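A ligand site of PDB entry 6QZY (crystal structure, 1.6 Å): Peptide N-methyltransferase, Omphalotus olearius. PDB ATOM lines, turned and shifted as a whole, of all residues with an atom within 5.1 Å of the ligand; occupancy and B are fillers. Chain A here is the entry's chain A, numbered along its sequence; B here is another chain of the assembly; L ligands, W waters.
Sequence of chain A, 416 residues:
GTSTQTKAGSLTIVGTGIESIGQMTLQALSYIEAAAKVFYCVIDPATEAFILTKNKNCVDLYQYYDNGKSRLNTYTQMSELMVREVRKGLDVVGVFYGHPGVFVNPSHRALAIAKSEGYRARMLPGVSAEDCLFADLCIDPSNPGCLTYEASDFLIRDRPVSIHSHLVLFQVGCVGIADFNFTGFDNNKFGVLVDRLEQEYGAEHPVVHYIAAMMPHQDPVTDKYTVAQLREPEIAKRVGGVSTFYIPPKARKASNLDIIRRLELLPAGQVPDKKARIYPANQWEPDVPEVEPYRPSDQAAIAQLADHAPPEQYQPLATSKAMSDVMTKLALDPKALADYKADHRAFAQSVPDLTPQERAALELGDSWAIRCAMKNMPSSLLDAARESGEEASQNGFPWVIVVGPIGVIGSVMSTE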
ATOM      1  N   ILE A  18     -13.219 -20.305   5.697  1.00  0.00           N
ATOM      2  CA  ILE A  18     -14.685 -20.149   5.840  1.00  0.00           C
ATOM      3  C   ILE A  18     -15.221 -19.306   4.683  1.00  0.00           C
ATOM      4  O   ILE A  18     -16.208 -19.712   4.039  1.00  0.00           O
ATOM      5  CB  ILE A  18     -15.029 -19.552   7.211  1.00  0.00           C
ATOM      6  CG1 ILE A  18     -14.568 -20.468   8.368  1.00  0.00           C
ATOM      7  CG2 ILE A  18     -16.501 -19.210   7.301  1.00  0.00           C
ATOM      8  CD1 ILE A  18     -15.252 -21.824   8.383  1.00  0.00           C
ATOM      9  N   ILE A  43     -18.739 -25.641   1.968  1.00  0.00           N
ATOM     10  CA  ILE A  43     -19.860 -24.876   2.605  1.00  0.00           C
ATOM     11  C   ILE A  43     -20.421 -23.838   1.621  1.00  0.00           C
ATOM     12  O   ILE A  43     -21.344 -23.105   2.021  1.00  0.00           O
ATOM     13  CB  ILE A  43     -19.297 -24.233   3.892  1.00  0.00           C
ATOM     14  CG1 ILE A  43     -20.388 -23.938   4.928  1.00  0.00           C
ATOM     15  CG2 ILE A  43     -18.427 -23.005   3.599  1.00  0.00           C
ATOM     16  CD1 ILE A  43     -20.878 -25.160   5.633  1.00  0.00           C
ATOM     17  N   TYR A  97     -13.981 -27.724   4.632  1.00  0.00           N
ATOM     18  CA  TYR A  97     -14.067 -26.268   4.834  1.00  0.00           C
ATOM     19  C   TYR A  97     -13.493 -25.893   6.204  1.00  0.00           C
ATOM     20  O   TYR A  97     -13.463 -26.688   7.187  1.00  0.00           O
ATOM     21  CB  TYR A  97     -15.471 -25.760   4.623  1.00  0.00           C
ATOM     22  CG  TYR A  97     -16.421 -26.063   5.731  1.00  0.00           C
ATOM     23  CD1 TYR A  97     -17.129 -27.259   5.767  1.00  0.00           C
ATOM     24  CD2 TYR A  97     -16.665 -25.121   6.716  1.00  0.00           C
ATOM     25  CE1 TYR A  97     -18.051 -27.495   6.779  1.00  0.00           C
ATOM     26  CE2 TYR A  97     -17.559 -25.355   7.734  1.00  0.00           C
ATOM     27  CZ  TYR A  97     -18.259 -26.542   7.764  1.00  0.00           C
ATOM     28  OH  TYR A  97     -19.178 -26.746   8.760  1.00  0.00           O
ATOM     29  N   GLY A  98     -13.066 -24.642   6.273  1.00  0.00           N
ATOM     30  CA  GLY A  98     -12.375 -24.082   7.432  1.00  0.00           C
ATOM     31  C   GLY A  98     -11.008 -24.713   7.623  1.00  0.00           C
ATOM     32  O   GLY A  98     -10.230 -24.760   6.674  1.00  0.00           O
ATOM     33  N   HIS A  99     -10.727 -25.119   8.850  1.00  0.00           N
ATOM     34  CA  HIS A  99      -9.567 -25.951   9.237  1.00  0.00           C
ATOM     35  C   HIS A  99     -10.040 -27.391   9.198  1.00  0.00           C
ATOM     36  O   HIS A  99     -11.034 -27.727   9.850  1.00  0.00           O
ATOM     37  CB  HIS A  99      -9.113 -25.559  10.642  1.00  0.00           C
ATOM     38  CG  HIS A  99      -7.881 -26.231  11.127  1.00  0.00           C
ATOM     39  ND1 HIS A  99      -7.696 -27.609  11.110  1.00  0.00           N
ATOM     40  CD2 HIS A  99      -6.787 -25.706  11.724  1.00  0.00           C
ATOM     41  CE1 HIS A  99      -6.551 -27.893  11.679  1.00  0.00           C
ATOM     42  NE2 HIS A  99      -5.969 -26.742  12.073  1.00  0.00           N
ATOM     43  N   PRO A 100      -9.350 -28.273   8.453  1.00  0.00           N
ATOM     44  CA  PRO A 100      -9.884 -29.623   8.236  1.00  0.00           C
ATOM     45  C   PRO A 100      -9.774 -30.556   9.446  1.00  0.00           C
ATOM     46  O   PRO A 100     -10.249 -31.666   9.358  1.00  0.00           O
ATOM     47  CB  PRO A 100      -9.002 -30.133   7.079  1.00  0.00           C
ATOM     48  CG  PRO A 100      -7.671 -29.465   7.353  1.00  0.00           C
ATOM     49  CD  PRO A 100      -8.061 -28.058   7.772  1.00  0.00           C
ATOM     50  N   VAL A 102     -10.482 -29.146  12.723  1.00  0.00           N
ATOM     51  CA  VAL A 102     -11.210 -28.406  13.790  1.00  0.00           C
ATOM     52  C   VAL A 102     -12.676 -28.768  13.637  1.00  0.00           C
ATOM     53  O   VAL A 102     -13.324 -28.372  12.660  1.00  0.00           O
ATOM     54  CB  VAL A 102     -10.933 -26.888  13.687  1.00  0.00           C
ATOM     55  CG1 VAL A 102     -11.889 -26.031  14.507  1.00  0.00           C
ATOM     56  CG2 VAL A 102      -9.495 -26.579  14.044  1.00  0.00           C
ATOM     57  N   PHE A 103     -13.178 -29.572  14.576  1.00  0.00           N
ATOM     58  CA  PHE A 103     -14.576 -30.053  14.557  1.00  0.00           C
ATOM     59  C   PHE A 103     -14.803 -30.860  13.265  1.00  0.00           C
ATOM     60  O   PHE A 103     -15.806 -30.640  12.596  1.00  0.00           O
ATOM     61  CB  PHE A 103     -15.557 -28.877  14.723  1.00  0.00           C
ATOM     62  CG  PHE A 103     -15.537 -28.256  16.098  1.00  0.00           C
ATOM     63  CD1 PHE A 103     -14.486 -27.465  16.509  1.00  0.00           C
ATOM     64  CD2 PHE A 103     -16.588 -28.474  16.985  1.00  0.00           C
ATOM     65  CE1 PHE A 103     -14.449 -26.914  17.783  1.00  0.00           C
ATOM     66  CE2 PHE A 103     -16.543 -27.929  18.259  1.00  0.00           C
ATOM     67  CZ  PHE A 103     -15.496 -27.144  18.658  1.00  0.00           C
ATOM     68  N   VAL A 104     -13.894 -31.786  12.945  1.00  0.00           N
ATOM     69  CA  VAL A 104     -14.023 -32.708  11.784  1.00  0.00           C
ATOM     70  C   VAL A 104     -13.600 -34.117  12.231  1.00  0.00           C
ATOM     71  O   VAL A 104     -12.453 -34.298  12.629  1.00  0.00           O
ATOM     72  CB  VAL A 104     -13.198 -32.258  10.554  1.00  0.00           C
ATOM     73  CG1 VAL A 104     -13.425 -33.204   9.386  1.00  0.00           C
ATOM     74  CG2 VAL A 104     -13.501 -30.830  10.121  1.00  0.00           C
ATOM     75  N   VAL A 127      -7.902 -21.819   8.066  1.00  0.00           N
ATOM     76  CA  VAL A 127      -8.610 -20.769   8.835  1.00  0.00           C
ATOM     77  C   VAL A 127      -9.938 -21.349   9.319  1.00  0.00           C
ATOM     78  O   VAL A 127     -10.793 -21.672   8.492  1.00  0.00           O
ATOM     79  CB  VAL A 127      -8.812 -19.528   7.967  1.00  0.00           C
ATOM     80  CG1 VAL A 127      -9.705 -18.518   8.672  1.00  0.00           C
ATOM     81  CG2 VAL A 127      -7.470 -18.936   7.563  1.00  0.00           C
ATOM     82  N   SER A 128     -10.117 -21.465  10.624  1.00  0.00           N
ATOM     83  CA  SER A 128     -11.358 -22.004  11.241  1.00  0.00           C
ATOM     84  C   SER A 128     -12.413 -20.908  11.458  1.00  0.00           C
ATOM     85  O   SER A 128     -12.116 -19.691  11.362  1.00  0.00           O
ATOM     86  CB  SER A 128     -11.045 -22.655  12.550  1.00  0.00           C
ATOM     87  OG  SER A 128     -10.796 -21.661  13.544  1.00  0.00           O
ATOM     88  N   ALA A 129     -13.619 -21.332  11.801  1.00  0.00           N
ATOM     89  CA  ALA A 129     -14.713 -20.415  12.187  1.00  0.00           C
ATOM     90  C   ALA A 129     -14.300 -19.641  13.448  1.00  0.00           C
ATOM     91  O   ALA A 129     -14.744 -18.489  13.591  1.00  0.00           O
ATOM     92  CB  ALA A 129     -15.990 -21.173  12.393  1.00  0.00           C
ATOM     93  N   GLU A 130     -13.500 -20.243  14.325  1.00  0.00           N
ATOM     94  CA  GLU A 130     -13.047 -19.551  15.540  1.00  0.00           C
ATOM     95  C   GLU A 130     -12.037 -18.452  15.146  1.00  0.00           C
ATOM     96  O   GLU A 130     -12.096 -17.347  15.724  1.00  0.00           O
ATOM     97  CB  GLU A 130     -12.435 -20.528  16.536  1.00  0.00           C
ATOM     98  CG  GLU A 130     -12.011 -19.834  17.807  1.00  0.00           C
ATOM     99  CD  GLU A 130     -11.709 -20.751  18.953  1.00  0.00           C
ATOM    100  OE1 GLU A 130     -10.570 -21.228  19.049  1.00  0.00           O
ATOM    101  OE2 GLU A 130     -12.627 -20.978  19.758  1.00  0.00           O
ATOM    102  N   LEU A 169     -18.772 -21.578  21.632  1.00  0.00           N
ATOM    103  CA  LEU A 169     -19.562 -22.824  21.440  1.00  0.00           C
ATOM    104  C   LEU A 169     -19.894 -23.020  19.963  1.00  0.00           C
ATOM    105  O   LEU A 169     -20.601 -22.177  19.391  1.00  0.00           O
ATOM    106  CB  LEU A 169     -20.831 -22.760  22.298  1.00  0.00           C
ATOM    107  CG  LEU A 169     -20.641 -22.633  23.800  1.00  0.00           C
ATOM    108  CD1 LEU A 169     -21.988 -22.572  24.512  1.00  0.00           C
ATOM    109  CD2 LEU A 169     -19.812 -23.784  24.363  1.00  0.00           C
ATOM    110  N   PHE A 170     -19.433 -24.132  19.392  1.00  0.00           N
ATOM    111  CA  PHE A 170     -19.726 -24.565  18.000  1.00  0.00           C
ATOM    112  C   PHE A 170     -20.972 -25.467  18.022  1.00  0.00           C
ATOM    113  O   PHE A 170     -21.226 -26.125  19.038  1.00  0.00           O
ATOM    114  CB  PHE A 170     -18.566 -25.385  17.427  1.00  0.00           C
ATOM    115  CG  PHE A 170     -17.370 -24.640  16.895  1.00  0.00           C
ATOM    116  CD1 PHE A 170     -16.610 -23.826  17.728  1.00  0.00           C
ATOM    117  CD2 PHE A 170     -16.948 -24.828  15.591  1.00  0.00           C
ATOM    118  CE1 PHE A 170     -15.489 -23.165  17.226  1.00  0.00           C
ATOM    119  CE2 PHE A 170     -15.828 -24.183  15.097  1.00  0.00           C
ATOM    120  CZ  PHE A 170     -15.102 -23.349  15.914  1.00  0.00           C
ATOM    121  N   GLN A 171     -21.687 -25.525  16.899  1.00  0.00           N
ATOM    122  CA  GLN A 171     -22.785 -26.517  16.661  1.00  0.00           C
ATOM    123  C   GLN A 171     -23.939 -26.241  17.636  1.00  0.00           C
ATOM    124  O   GLN A 171     -24.633 -27.190  18.020  1.00  0.00           O
ATOM    125  CB  GLN A 171     -22.250 -27.954  16.723  1.00  0.00           C
ATOM    126  CG  GLN A 171     -21.091 -28.163  15.740  1.00  0.00           C
ATOM    127  CD  GLN A 171     -20.870 -29.551  15.208  1.00  0.00           C
ATOM    128  OE1 GLN A 171     -20.328 -29.711  14.106  1.00  0.00           O
ATOM    129  NE2 GLN A 171     -21.249 -30.560  15.966  1.00  0.00           N
ATOM    130  N   VAL A 172     -24.202 -24.967  17.918  1.00  0.00           N
ATOM    131  CA  VAL A 172     -25.327 -24.546  18.800  1.00  0.00           C
ATOM    132  C   VAL A 172     -26.667 -24.728  18.071  1.00  0.00           C
ATOM    133  O   VAL A 172     -27.711 -24.686  18.752  1.00  0.00           O
ATOM    134  CB  VAL A 172     -25.142 -23.114  19.338  1.00  0.00           C
ATOM    135  CG1 VAL A 172     -23.956 -23.023  20.284  1.00  0.00           C
ATOM    136  CG2 VAL A 172     -25.005 -22.081  18.219  1.00  0.00           C
ATOM    137  N   TYR A 210     -22.884 -15.465  16.233  1.00  0.00           N
ATOM    138  CA  TYR A 210     -21.847 -15.187  15.216  1.00  0.00           C
ATOM    139  C   TYR A 210     -22.037 -16.110  14.009  1.00  0.00           C
ATOM    140  O   TYR A 210     -22.042 -17.350  14.145  1.00  0.00           O
ATOM    141  CB  TYR A 210     -20.449 -15.341  15.820  1.00  0.00           C
ATOM    142  CG  TYR A 210     -19.381 -15.137  14.788  1.00  0.00           C
ATOM    143  CD1 TYR A 210     -19.257 -13.919  14.136  1.00  0.00           C
ATOM    144  CD2 TYR A 210     -18.528 -16.167  14.404  1.00  0.00           C
ATOM    145  CE1 TYR A 210     -18.309 -13.726  13.145  1.00  0.00           C
ATOM    146  CE2 TYR A 210     -17.575 -15.983  13.424  1.00  0.00           C
ATOM    147  CZ  TYR A 210     -17.447 -14.754  12.806  1.00  0.00           C
ATOM    148  OH  TYR A 210     -16.519 -14.568  11.840  1.00  0.00           O
ATOM    149  N   ILE A 211     -22.131 -15.494  12.823  1.00  0.00           N
ATOM    150  CA  ILE A 211     -22.005 -16.212  11.532  1.00  0.00           C
ATOM    151  C   ILE A 211     -21.024 -15.424  10.671  1.00  0.00           C
ATOM    152  O   ILE A 211     -21.323 -14.258  10.320  1.00  0.00           O
ATOM    153  CB  ILE A 211     -23.353 -16.432  10.816  1.00  0.00           C
ATOM    154  CG1 ILE A 211     -24.408 -17.037  11.742  1.00  0.00           C
ATOM    155  CG2 ILE A 211     -23.120 -17.281   9.572  1.00  0.00           C
ATOM    156  CD1 ILE A 211     -25.797 -17.138  11.119  1.00  0.00           C
ATOM    157  N   ALA A 212     -19.865 -16.019  10.396  1.00  0.00           N
ATOM    158  CA  ALA A 212     -18.863 -15.478   9.467  1.00  0.00           C
ATOM    159  C   ALA A 212     -19.503 -15.404   8.082  1.00  0.00           C
ATOM    160  O   ALA A 212     -20.229 -16.369   7.683  1.00  0.00           O
ATOM    161  CB  ALA A 212     -17.635 -16.341   9.469  1.00  0.00           C
ATOM    162  N   MET A 214     -19.745 -16.026   4.329  1.00  0.00           N
ATOM    163  CA  MET A 214     -19.199 -17.120   3.490  1.00  0.00           C
ATOM    164  C   MET A 214     -18.967 -16.617   2.076  1.00  0.00           C
ATOM    165  O   MET A 214     -18.155 -17.212   1.368  1.00  0.00           O
ATOM    166  CB  MET A 214     -20.145 -18.334   3.515  1.00  0.00           C
ATOM    167  CG  MET A 214     -19.963 -19.078   4.817  1.00  0.00           C
ATOM    168  SD  MET A 214     -21.315 -20.190   5.237  1.00  0.00           S
ATOM    169  CE  MET A 214     -22.620 -19.015   5.571  1.00  0.00           C
ATOM    170  N   GLY A 241     -27.179 -24.095  11.093  1.00  0.00           N
ATOM    171  CA  GLY A 241     -26.063 -25.054  10.913  1.00  0.00           C
ATOM    172  C   GLY A 241     -24.706 -24.397  10.984  1.00  0.00           C
ATOM    173  O   GLY A 241     -23.726 -25.112  11.271  1.00  0.00           O
ATOM    174  N   VAL A 242     -24.612 -23.103  10.692  1.00  0.00           N
ATOM    175  CA  VAL A 242     -23.290 -22.397  10.636  1.00  0.00           C
ATOM    176  C   VAL A 242     -23.232 -21.333  11.749  1.00  0.00           C
ATOM    177  O   VAL A 242     -22.379 -20.422  11.660  1.00  0.00           O
ATOM    178  CB  VAL A 242     -23.010 -21.805   9.238  1.00  0.00           C
ATOM    179  CG1 VAL A 242     -22.727 -22.919   8.234  1.00  0.00           C
ATOM    180  CG2 VAL A 242     -24.128 -20.890   8.751  1.00  0.00           C
ATOM    181  N   SER A 243     -24.097 -21.455  12.763  1.00  0.00           N
ATOM    182  CA  SER A 243     -24.159 -20.540  13.925  1.00  0.00           C
ATOM    183  C   SER A 243     -23.151 -20.966  14.990  1.00  0.00           C
ATOM    184  O   SER A 243     -23.081 -22.169  15.328  1.00  0.00           O
ATOM    185  CB  SER A 243     -25.534 -20.480  14.525  1.00  0.00           C
ATOM    186  OG  SER A 243     -26.444 -19.838  13.637  1.00  0.00           O
ATOM    187  N   THR A 244     -22.424 -19.983  15.518  1.00  0.00           N
ATOM    188  CA  THR A 244     -21.490 -20.146  16.650  1.00  0.00           C
ATOM    189  C   THR A 244     -21.880 -19.133  17.724  1.00  0.00           C
ATOM    190  O   THR A 244     -22.308 -18.029  17.351  1.00  0.00           O
ATOM    191  CB  THR A 244     -20.033 -19.985  16.181  1.00  0.00           C
ATOM    192  OG1 THR A 244     -19.743 -21.101  15.346  1.00  0.00           O
ATOM    193  CG2 THR A 244     -19.024 -19.909  17.299  1.00  0.00           C
ATOM    194  N   MVA B   6     -23.507 -28.349   7.165  1.00  0.00           N
ATOM    195  CN  MVA B   6     -23.139 -27.080   7.775  1.00  0.00           C
ATOM    196  CA  MVA B   6     -22.391 -29.277   6.866  1.00  0.00           C
ATOM    197  CB  MVA B   6     -21.447 -28.714   5.790  1.00  0.00           C
ATOM    198  CG1 MVA B   6     -20.467 -29.791   5.326  1.00  0.00           C
ATOM    199  CG2 MVA B   6     -22.248 -28.184   4.607  1.00  0.00           C
ATOM    200  C   MVA B   6     -21.681 -29.584   8.187  1.00  0.00           C
ATOM    201  O   MVA B   6     -20.716 -28.903   8.538  1.00  0.00           O
ATOM    202  N   ILE B   7     -22.238 -30.544   8.909  1.00  0.00           N
ATOM    203  CA  ILE B   7     -21.809 -30.912  10.285  1.00  0.00           C
ATOM    204  C   ILE B   7     -20.888 -32.122  10.160  1.00  0.00           C
ATOM    205  O   ILE B   7     -21.354 -33.174   9.718  1.00  0.00           O
ATOM    206  CB  ILE B   7     -23.031 -31.191  11.170  1.00  0.00           C
ATOM    207  CG1 ILE B   7     -23.989 -29.992  11.189  1.00  0.00           C
ATOM    208  CG2 ILE B   7     -22.601 -31.618  12.557  1.00  0.00           C
ATOM    209  CD1 ILE B   7     -23.359 -28.694  11.694  1.00  0.00           C
ATOM    210  N   MVA B   8     -19.596 -31.989  10.481  1.00  0.00           N
ATOM    211  CN  MVA B   8     -19.005 -30.782  11.096  1.00  0.00           C
ATOM    212  CA  MVA B   8     -18.672 -33.110  10.184  1.00  0.00           C
ATOM    213  CB  MVA B   8     -17.657 -32.729   9.085  1.00  0.00           C
ATOM    214  CG1 MVA B   8     -17.234 -33.945   8.299  1.00  0.00           C
ATOM    215  CG2 MVA B   8     -18.183 -31.662   8.126  1.00  0.00           C
ATOM    216  C   MVA B   8     -17.990 -33.643  11.450  1.00  0.00           C
ATOM    217  O   MVA B   8     -16.925 -34.232  11.362  1.00  0.00           O
ATOM    218  N   VAL B   9     -18.635 -33.474  12.610  1.00  0.00           N
ATOM    219  CA  VAL B   9     -18.165 -34.035  13.912  1.00  0.00           C
ATOM    220  C   VAL B   9     -19.384 -34.216  14.814  1.00  0.00           C
ATOM    221  O   VAL B   9     -20.404 -33.522  14.597  1.00  0.00           O
ATOM    222  CB  VAL B   9     -17.099 -33.133  14.566  1.00  0.00           C
ATOM    223  CG1 VAL B   9     -17.710 -31.933  15.260  1.00  0.00           C
ATOM    224  CG2 VAL B   9     -16.216 -33.903  15.530  1.00  0.00           C
HETATM  225  N1  LIG L   1     -13.926 -27.258  10.277  1.00  0.00           N
HETATM  226  C1  LIG L   1     -14.828 -26.089  10.505  1.00  0.00           C
HETATM  227  C2  LIG L   1     -15.892 -26.391  11.573  1.00  0.00           C
HETATM  228  C3  LIG L   1     -16.778 -27.571  11.201  1.00  0.00           C
HETATM  229  S1  LIG L   1     -18.001 -27.985  12.481  1.00  0.00           S
HETATM  230  C4  LIG L   1     -13.985 -24.899  10.982  1.00  0.00           C
HETATM  231  O1  LIG L   1     -14.521 -23.941  11.519  1.00  0.00           O
HETATM  232  O2  LIG L   1     -12.782 -24.965  10.808  1.00  0.00           O
HETATM  233  C5  LIG L   1     -19.447 -26.944  12.119  1.00  0.00           C
HETATM  234  C6  LIG L   1     -19.618 -25.771  13.046  1.00  0.00           C
HETATM  235  O3  LIG L   1     -18.635 -24.755  12.715  1.00  0.00           O
HETATM  236  C7  LIG L   1     -20.937 -25.011  12.942  1.00  0.00           C
HETATM  237  O4  LIG L   1     -22.015 -25.628  13.629  1.00  0.00           O
HETATM  238  C8  LIG L   1     -20.551 -23.671  13.579  1.00  0.00           C
HETATM  239  O5  LIG L   1     -20.493 -23.711  14.988  1.00  0.00           O
HETATM  240  C9  LIG L   1     -19.162 -23.469  12.964  1.00  0.00           C
HETATM  241  N2  LIG L   1     -19.220 -22.712  11.717  1.00  0.00           N
HETATM  242  C10 LIG L   1     -19.208 -23.177  10.429  1.00  0.00           C
HETATM  243  N3  LIG L   1     -19.330 -22.231   9.531  1.00  0.00           N
HETATM  244  C11 LIG L   1     -19.465 -21.071  10.267  1.00  0.00           C
HETATM  245  C12 LIG L   1     -19.656 -19.719   9.902  1.00  0.00           C
HETATM  246  N4  LIG L   1     -19.765 -19.303   8.636  1.00  0.00           N
HETATM  247  N5  LIG L   1     -19.754 -18.806  10.898  1.00  0.00           N
HETATM  248  C13 LIG L   1     -19.666 -19.233  12.166  1.00  0.00           C
HETATM  249  N6  LIG L   1     -19.501 -20.478  12.627  1.00  0.00           N
HETATM  250  C14 LIG L   1     -19.411 -21.355  11.624  1.00  0.00           C
HETATM  251  O   HOH W   1     -24.604 -24.402  14.742  1.00  0.00           O
HETATM  252  O   HOH W   2     -15.045 -28.624   7.974  1.00  0.00           O
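N1 of the ligand sits at hydrogen-bond distance from O of Val 102, 2.7 Å away. OG1 of Thr 244 is in hydrogen-bond range of O5 of the ligand, 2.7 Å away. The backbone NH of Ala 129 sits at hydrogen-bond distance from an oxygen (O1) of the ligand (2.8 Å). N of Ala 212 lies within hydrogen-bond range of N5 of the ligand, at 2.8 Å. N4 of the ligand sits at hydrogen-bond distance from O of Ala 212 (3.1 Å). The backbone NH (N) of His 99 sits at hydrogen-bond distance from an oxygen (O2) of the ligand (2.8 Å). The backbone carbonyl oxygen of His 99 is in hydrogen-bond range of a nitrogen (N1) of the ligand (3.0 Å). The backbone NH of Gln 171 sits at hydrogen-bond distance from an oxygen (O5) of the ligand. OE1 of Gln 171 lies close to S1 of the ligand (3.3 Å). The backbone carbonyl oxygen (O) of Gly 241 lies within hydrogen-bond range of an oxygen (O4) of the ligand (3.0 Å). The backbone carbonyl oxygen (O) of Ser 243 is in hydrogen-bond range of an oxygen (O5) of the ligand (3.0 Å). N1 of the ligand sits at hydrogen-bond distance from O of Tyr 97 (3.2 Å).
The backbone carbonyl oxygen (O) of Thr 244 sits at hydrogen-bond distance from the backbone NH (N) of Tyr 210, 2.9 Å away. The backbone carbonyl oxygen (O) of Val 127 is in hydrogen-bond range of the backbone NH (N) of His 99 (3.5 Å). The side-chain amide nitrogen (NE2) of Gln 171 sits at hydrogen-bond distance from the backbone carbonyl oxygen (O) of Val 9 of chain B, 3.4 Å away. OH of Tyr 97 is in hydrogen-bond range of O of MVA 6 of chain B (2.7 Å). The side-chain hydroxyl of Ser 128 sits close to the backbone NH of Glu 130.
The backbone carbonyl oxygen of Phe 103 lies close to a sulfur (S1) of the ligand (3.4 Å). O of Val 242 sits close to N6 of the ligand (3.0 Å). Ile 18 touches the ligand (CG2 to N4, 3.5 Å). CA of Gly 98 touches O2 of the ligand (3.5 Å). Val 104 touches the ligand (CG2 to N1, 3.6 Å). CA of Ser 128 touches O2 of the ligand (3.3 Å). CA of Phe 170 touches O5 of the ligand (3.2 Å). Tyr 210 touches the ligand (O to C13, 3.6 Å). Ile 211 touches the ligand. CG of Met 214 touches N4 of the ligand (3.8 Å). CD1 of Ile 7 of chain B touches O4 of the ligand, at 3.9 Å. CN of MVA 8 of chain B touches S1 of the ligand, at 3.3 Å. Hydrophobic or aromatic side chains within 4 Å of the ligand: Ile 18, Tyr 97, His 99, Val 102, Phe 103, Val 104, Ala 129, Phe 170, Tyr 210, Ile 211, Ala 212, Met 214, Val 242 and Ile 7 of chain B. Within 4 Å of the ligand: Ile 18, Tyr 97, Gly 98, His 99, Val 102, Phe 103, Val 104, Ser 128, Ala 129, Phe 170, Gln 171, Tyr 210, Ile 211, Ala 212, Met 214, Gly 241, Val 242, Ser 243, Thr 244, Ile 7 of chain B and MVA 8 of chain B.
Water W2 lies within hydrogen-bond range of the backbone carbonyl oxygen (O) of Tyr 97 (2.6 Å) and a nitrogen (N1) of the ligand (2.9 Å). Water W1 lies within hydrogen-bond range of the backbone carbonyl oxygen (O) of Ser 243, an oxygen (O4) of the ligand and the backbone NH (N) of Val 172.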
